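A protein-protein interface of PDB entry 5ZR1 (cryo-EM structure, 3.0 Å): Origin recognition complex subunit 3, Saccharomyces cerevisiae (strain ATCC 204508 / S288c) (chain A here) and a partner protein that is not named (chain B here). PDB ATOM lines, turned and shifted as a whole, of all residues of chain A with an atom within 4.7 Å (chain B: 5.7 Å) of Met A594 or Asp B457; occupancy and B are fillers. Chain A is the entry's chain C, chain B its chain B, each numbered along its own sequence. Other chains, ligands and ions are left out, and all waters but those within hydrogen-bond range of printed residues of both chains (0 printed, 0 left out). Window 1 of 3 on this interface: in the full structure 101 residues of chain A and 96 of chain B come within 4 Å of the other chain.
Printed residues of chain B that touch a printed residue of chain A: Val B319, Asp B457, His B458 and Ile B459. Hydrophobic or aromatic side chains of chain B that line the printed part of chain A: Val B319, His B458 and Ile B459. Among the printed residues, no Asp or Glu carboxylate lies within 4 Å of a Lys or Arg side-chain nitrogen of the other chain.
Val B319 touches Leu A521 (CG2 to CD1, 3.8 Å). Asn A593 touches His B458. CE of Met A594 touches CG2 of Val B319, at 3.7 Å. O of Asp B457 touches CG of Met A594 (3.9 Å). Gly A595 touches His B458 (CA to NE2, 3.4 Å). CD2 of Leu A596 touches CD1 of Ile B459, 3.7 Å away.
Met A594 touches just these residues of chain B: Val B319, Asp B457, His B458 and Ile B459. Asp B457 touches just one residue of chain A: Met A594. Of the printed residues of chain B, Gly A595 touches His B458. Of the printed residues of chain B, Leu A521 touches Val B319 (3.8 Å). Of the printed residues of chain A, Val B319 touches Leu A521 (3.8 Å) and Met A594 (3.7 Å). The nearest residue of chain B that does not touch Met A594 is Gly B320 (4.2 Å). The nearest printed residue of chain B that does not touch Asn A593 is Asp B457 (4.5 Å).
A ring nitrogen (ND1) of His B458 sits at hydrogen-bond distance from the backbone NH of Tyr B460 (3.0 Å). The backbone NH (N) of His B458 lies within hydrogen-bond range of the side-chain carboxylate (OD2) of Asp B428, at 2.6 Å. OD1 of Asp B428 sits at hydrogen-bond distance from N of Asp B457 (3.1 Å). OD2 of Asp B457 lies close to OD1 of Asn B426 (2.8 Å). The backbone carbonyl oxygen (O) of Phe A591 lies within hydrogen-bond range of the backbone NH (N) of Leu A596 (2.9 Å). The side-chain amide oxygen (OD1) of Asn A593 lies close to the backbone carbonyl oxygen (O) of Ala A590 (3.0 Å).
The backbone NH of Ile B459 lies within hydrogen-bond range of the backbone carbonyl oxygen of Met A594 (2.8 Å). O of Met A594 lies close to ND1 of His B458 (3.5 Å).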
ATOM      1  N   LEU A 521     -13.131   7.940  28.611  1.00  0.00           N
ATOM      2  CA  LEU A 521     -14.199   8.068  27.628  1.00  0.00           C
ATOM      3  C   LEU A 521     -14.340   9.500  27.131  1.00  0.00           C
ATOM      4  O   LEU A 521     -14.737   9.717  25.983  1.00  0.00           O
ATOM      5  CB  LEU A 521     -15.520   7.584  28.214  1.00  0.00           C
ATOM      6  CG  LEU A 521     -15.588   6.090  28.500  1.00  0.00           C
ATOM      7  CD1 LEU A 521     -16.915   5.730  29.136  1.00  0.00           C
ATOM      8  CD2 LEU A 521     -15.372   5.322  27.222  1.00  0.00           C
ATOM      9  N   ALA A 590     -15.741   0.318  25.144  1.00  0.00           N
ATOM     10  CA  ALA A 590     -16.937   0.977  25.641  1.00  0.00           C
ATOM     11  C   ALA A 590     -17.602   1.817  24.563  1.00  0.00           C
ATOM     12  O   ALA A 590     -18.812   2.044  24.626  1.00  0.00           O
ATOM     13  CB  ALA A 590     -16.601   1.836  26.857  1.00  0.00           C
ATOM     14  N   PHE A 591     -16.850   2.270  23.563  1.00  0.00           N
ATOM     15  CA  PHE A 591     -17.462   2.988  22.455  1.00  0.00           C
ATOM     16  C   PHE A 591     -18.133   2.078  21.443  1.00  0.00           C
ATOM     17  O   PHE A 591     -18.856   2.585  20.582  1.00  0.00           O
ATOM     18  CB  PHE A 591     -16.442   3.861  21.725  1.00  0.00           C
ATOM     19  CG  PHE A 591     -16.123   5.148  22.424  1.00  0.00           C
ATOM     20  CD1 PHE A 591     -16.863   5.566  23.516  1.00  0.00           C
ATOM     21  CD2 PHE A 591     -15.110   5.963  21.956  1.00  0.00           C
ATOM     22  CE1 PHE A 591     -16.578   6.757  24.143  1.00  0.00           C
ATOM     23  CE2 PHE A 591     -14.822   7.154  22.580  1.00  0.00           C
ATOM     24  CZ  PHE A 591     -15.557   7.550  23.673  1.00  0.00           C
ATOM     25  N   GLU A 592     -17.926   0.764  21.506  1.00  0.00           N
ATOM     26  CA  GLU A 592     -18.629  -0.083  20.551  1.00  0.00           C
ATOM     27  C   GLU A 592     -20.030  -0.433  21.036  1.00  0.00           C
ATOM     28  O   GLU A 592     -20.997  -0.303  20.280  1.00  0.00           O
ATOM     29  CB  GLU A 592     -17.854  -1.358  20.251  1.00  0.00           C
ATOM     30  CG  GLU A 592     -18.571  -2.160  19.178  1.00  0.00           C
ATOM     31  CD  GLU A 592     -17.885  -3.442  18.831  1.00  0.00           C
ATOM     32  OE1 GLU A 592     -16.834  -3.714  19.430  1.00  0.00           O
ATOM     33  OE2 GLU A 592     -18.408  -4.186  17.975  1.00  0.00           O
ATOM     34  N   ASN A 593     -20.175  -0.870  22.288  1.00  0.00           N
ATOM     35  CA  ASN A 593     -21.518  -1.221  22.734  1.00  0.00           C
ATOM     36  C   ASN A 593     -22.378  -0.004  23.063  1.00  0.00           C
ATOM     37  O   ASN A 593     -23.578  -0.168  23.297  1.00  0.00           O
ATOM     38  CB  ASN A 593     -21.475  -2.204  23.916  1.00  0.00           C
ATOM     39  CG  ASN A 593     -20.749  -1.670  25.135  1.00  0.00           C
ATOM     40  OD1 ASN A 593     -20.266  -0.540  25.165  1.00  0.00           O
ATOM     41  ND2 ASN A 593     -20.693  -2.494  26.172  1.00  0.00           N
ATOM     42  N   MET A 594     -21.802   1.200  23.087  1.00  0.00           N
ATOM     43  CA  MET A 594     -22.611   2.405  22.962  1.00  0.00           C
ATOM     44  C   MET A 594     -23.067   2.635  21.533  1.00  0.00           C
ATOM     45  O   MET A 594     -24.059   3.334  21.320  1.00  0.00           O
ATOM     46  CB  MET A 594     -21.842   3.641  23.419  1.00  0.00           C
ATOM     47  CG  MET A 594     -21.586   3.719  24.892  1.00  0.00           C
ATOM     48  SD  MET A 594     -20.651   5.201  25.291  1.00  0.00           S
ATOM     49  CE  MET A 594     -20.308   4.897  27.014  1.00  0.00           C
ATOM     50  N   GLY A 595     -22.365   2.078  20.558  1.00  0.00           N
ATOM     51  CA  GLY A 595     -22.726   2.242  19.172  1.00  0.00           C
ATOM     52  C   GLY A 595     -22.002   3.337  18.436  1.00  0.00           C
ATOM     53  O   GLY A 595     -22.494   3.778  17.394  1.00  0.00           O
ATOM     54  N   LEU A 596     -20.857   3.793  18.935  1.00  0.00           N
ATOM     55  CA  LEU A 596     -20.146   4.884  18.289  1.00  0.00           C
ATOM     56  C   LEU A 596     -19.155   4.409  17.238  1.00  0.00           C
ATOM     57  O   LEU A 596     -18.663   5.232  16.463  1.00  0.00           O
ATOM     58  CB  LEU A 596     -19.385   5.717  19.323  1.00  0.00           C
ATOM     59  CG  LEU A 596     -20.162   6.301  20.502  1.00  0.00           C
ATOM     60  CD1 LEU A 596     -19.264   7.154  21.356  1.00  0.00           C
ATOM     61  CD2 LEU A 596     -21.354   7.082  20.067  1.00  0.00           C
ATOM     62  N   GLY B 318     -27.155   7.772  29.918  1.00  0.00           N
ATOM     63  CA  GLY B 318     -25.931   8.462  30.257  1.00  0.00           C
ATOM     64  C   GLY B 318     -24.707   7.667  29.868  1.00  0.00           C
ATOM     65  O   GLY B 318     -24.819   6.541  29.376  1.00  0.00           O
ATOM     66  N   VAL B 319     -23.531   8.242  30.085  1.00  0.00           N
ATOM     67  CA  VAL B 319     -22.262   7.594  29.781  1.00  0.00           C
ATOM     68  C   VAL B 319     -21.669   7.024  31.067  1.00  0.00           C
ATOM     69  O   VAL B 319     -21.574   7.718  32.086  1.00  0.00           O
ATOM     70  CB  VAL B 319     -21.306   8.571  29.067  1.00  0.00           C
ATOM     71  CG1 VAL B 319     -21.269   9.919  29.751  1.00  0.00           C
ATOM     72  CG2 VAL B 319     -19.906   8.011  29.017  1.00  0.00           C
ATOM     73  N   GLY B 320     -21.318   5.746  31.035  1.00  0.00           N
ATOM     74  CA  GLY B 320     -20.816   5.041  32.196  1.00  0.00           C
ATOM     75  C   GLY B 320     -21.777   3.959  32.652  1.00  0.00           C
ATOM     76  O   GLY B 320     -22.907   3.846  32.186  1.00  0.00           O
ATOM     77  N   SER B 321     -21.290   3.153  33.592  1.00  0.00           N
ATOM     78  CA  SER B 321     -22.111   2.081  34.138  1.00  0.00           C
ATOM     79  C   SER B 321     -23.183   2.645  35.049  1.00  0.00           C
ATOM     80  O   SER B 321     -22.900   3.432  35.957  1.00  0.00           O
ATOM     81  CB  SER B 321     -21.268   1.082  34.914  1.00  0.00           C
ATOM     82  OG  SER B 321     -22.081   0.067  35.472  1.00  0.00           O
ATOM     83  N   LYS B 322     -24.417   2.229  34.810  1.00  0.00           N
ATOM     84  CA  LYS B 322     -25.550   2.631  35.621  1.00  0.00           C
ATOM     85  C   LYS B 322     -26.025   1.499  36.512  1.00  0.00           C
ATOM     86  O   LYS B 322     -27.089   1.608  37.117  1.00  0.00           O
ATOM     87  CB  LYS B 322     -26.669   3.113  34.705  1.00  0.00           C
ATOM     88  CG  LYS B 322     -26.279   4.337  33.912  1.00  0.00           C
ATOM     89  CD  LYS B 322     -27.298   4.638  32.859  1.00  0.00           C
ATOM     90  CE  LYS B 322     -27.145   3.651  31.732  1.00  0.00           C
ATOM     91  NZ  LYS B 322     -25.837   3.840  31.058  1.00  0.00           N
ATOM     92  N   ASN B 426     -29.663  -2.464  31.378  1.00  0.00           N
ATOM     93  CA  ASN B 426     -29.346  -2.476  29.948  1.00  0.00           C
ATOM     94  C   ASN B 426     -30.516  -3.010  29.118  1.00  0.00           C
ATOM     95  O   ASN B 426     -30.462  -4.088  28.535  1.00  0.00           O
ATOM     96  CB  ASN B 426     -28.060  -3.257  29.665  1.00  0.00           C
ATOM     97  CG  ASN B 426     -26.842  -2.503  30.093  1.00  0.00           C
ATOM     98  OD1 ASN B 426     -26.771  -1.293  29.918  1.00  0.00           O
ATOM     99  ND2 ASN B 426     -25.877  -3.200  30.662  1.00  0.00           N
ATOM    100  N   ASP B 428     -31.460  -2.085  26.347  1.00  0.00           N
ATOM    101  CA  ASP B 428     -31.029  -2.228  24.964  1.00  0.00           C
ATOM    102  C   ASP B 428     -29.845  -3.180  24.812  1.00  0.00           C
ATOM    103  O   ASP B 428     -29.070  -3.059  23.858  1.00  0.00           O
ATOM    104  CB  ASP B 428     -30.694  -0.855  24.395  1.00  0.00           C
ATOM    105  CG  ASP B 428     -29.709  -0.095  25.255  1.00  0.00           C
ATOM    106  OD1 ASP B 428     -29.312  -0.591  26.329  1.00  0.00           O
ATOM    107  OD2 ASP B 428     -29.338   1.023  24.862  1.00  0.00           O
ATOM    108  N   SER B 455     -32.665   0.927  32.261  1.00  0.00           N
ATOM    109  CA  SER B 455     -31.480   1.676  31.867  1.00  0.00           C
ATOM    110  C   SER B 455     -31.057   1.258  30.469  1.00  0.00           C
ATOM    111  O   SER B 455     -31.319   0.133  30.043  1.00  0.00           O
ATOM    112  CB  SER B 455     -30.316   1.465  32.834  1.00  0.00           C
ATOM    113  OG  SER B 455     -29.780   0.163  32.708  1.00  0.00           O
ATOM    114  N   THR B 456     -30.408   2.177  29.750  1.00  0.00           N
ATOM    115  CA  THR B 456     -29.965   1.938  28.379  1.00  0.00           C
ATOM    116  C   THR B 456     -28.578   2.523  28.155  1.00  0.00           C
ATOM    117  O   THR B 456     -28.278   3.620  28.631  1.00  0.00           O
ATOM    118  CB  THR B 456     -30.926   2.549  27.347  1.00  0.00           C
ATOM    119  OG1 THR B 456     -31.137   3.932  27.646  1.00  0.00           O
ATOM    120  CG2 THR B 456     -32.256   1.809  27.278  1.00  0.00           C
ATOM    121  N   ASP B 457     -27.741   1.800  27.405  1.00  0.00           N
ATOM    122  CA  ASP B 457     -26.406   2.275  27.055  1.00  0.00           C
ATOM    123  C   ASP B 457     -26.236   2.702  25.608  1.00  0.00           C
ATOM    124  O   ASP B 457     -25.440   3.605  25.351  1.00  0.00           O
ATOM    125  CB  ASP B 457     -25.341   1.211  27.352  1.00  0.00           C
ATOM    126  CG  ASP B 457     -24.916   1.194  28.803  1.00  0.00           C
ATOM    127  OD1 ASP B 457     -25.035   2.240  29.473  1.00  0.00           O
ATOM    128  OD2 ASP B 457     -24.413   0.149  29.260  1.00  0.00           O
ATOM    129  N   HIS B 458     -26.924   2.072  24.659  1.00  0.00           N
ATOM    130  CA  HIS B 458     -26.674   2.356  23.252  1.00  0.00           C
ATOM    131  C   HIS B 458     -27.227   3.729  22.895  1.00  0.00           C
ATOM    132  O   HIS B 458     -28.212   4.193  23.470  1.00  0.00           O
ATOM    133  CB  HIS B 458     -27.309   1.284  22.365  1.00  0.00           C
ATOM    134  CG  HIS B 458     -26.741   1.222  20.983  1.00  0.00           C
ATOM    135  ND1 HIS B 458     -27.054   2.137  20.006  1.00  0.00           N
ATOM    136  CD2 HIS B 458     -25.930   0.313  20.397  1.00  0.00           C
ATOM    137  CE1 HIS B 458     -26.426   1.822  18.889  1.00  0.00           C
ATOM    138  NE2 HIS B 458     -25.743   0.713  19.098  1.00  0.00           N
ATOM    139  N   ILE B 459     -26.568   4.391  21.947  1.00  0.00           N
ATOM    140  CA  ILE B 459     -26.910   5.775  21.653  1.00  0.00           C
ATOM    141  C   ILE B 459     -28.129   5.879  20.735  1.00  0.00           C
ATOM    142  O   ILE B 459     -28.814   6.910  20.741  1.00  0.00           O
ATOM    143  CB  ILE B 459     -25.658   6.486  21.104  1.00  0.00           C
ATOM    144  CG1 ILE B 459     -25.820   8.005  21.152  1.00  0.00           C
ATOM    145  CG2 ILE B 459     -25.323   6.007  19.710  1.00  0.00           C
ATOM    146  CD1 ILE B 459     -24.549   8.774  20.976  1.00  0.00           C
ATOM    147  N   TYR B 460     -28.463   4.829  19.985  1.00  0.00           N
ATOM    148  CA  TYR B 460     -29.697   4.796  19.214  1.00  0.00           C
ATOM    149  C   TYR B 460     -30.788   3.993  19.901  1.00  0.00           C
ATOM    150  O   TYR B 460     -31.650   3.438  19.220  1.00  0.00           O
ATOM    151  CB  TYR B 460     -29.471   4.221  17.816  1.00  0.00           C
ATOM    152  CG  TYR B 460     -28.502   4.994  16.976  1.00  0.00           C
ATOM    153  CD1 TYR B 460     -28.800   6.272  16.543  1.00  0.00           C
ATOM    154  CD2 TYR B 460     -27.314   4.420  16.561  1.00  0.00           C
ATOM    155  CE1 TYR B 460     -27.922   6.980  15.763  1.00  0.00           C
ATOM    156  CE2 TYR B 460     -26.430   5.116  15.775  1.00  0.00           C
ATOM    157  CZ  TYR B 460     -26.741   6.394  15.380  1.00  0.00           C
ATOM    158  OH  TYR B 460     -25.859   7.086  14.595  1.00  0.00           O
ATOM    159  N   ALA B 461     -30.733   3.867  21.217  1.00  0.00           N
ATOM    160  CA  ALA B 461     -31.780   3.219  22.006  1.00  0.00           C
ATOM    161  C   ALA B 461     -33.217   3.731  21.819  1.00  0.00           C
ATOM    162  O   ALA B 461     -34.131   2.903  21.890  1.00  0.00           O
ATOM    163  CB  ALA B 461     -31.417   3.283  23.490  1.00  0.00           C
ATOM    164  N   GLU B 489     -20.414  -5.514  33.134  1.00  0.00           N
ATOM    165  CA  GLU B 489     -20.872  -5.646  31.757  1.00  0.00           C
ATOM    166  C   GLU B 489     -19.746  -6.082  30.827  1.00  0.00           C
ATOM    167  O   GLU B 489     -20.010  -6.669  29.773  1.00  0.00           O
ATOM    168  CB  GLU B 489     -21.470  -4.327  31.273  1.00  0.00           C
ATOM    169  CG  GLU B 489     -22.803  -3.952  31.896  1.00  0.00           C
ATOM    170  CD  GLU B 489     -22.676  -3.249  33.231  1.00  0.00           C
ATOM    171  OE1 GLU B 489     -21.543  -3.044  33.704  1.00  0.00           O
ATOM    172  OE2 GLU B 489     -23.720  -2.881  33.804  1.00  0.00           O
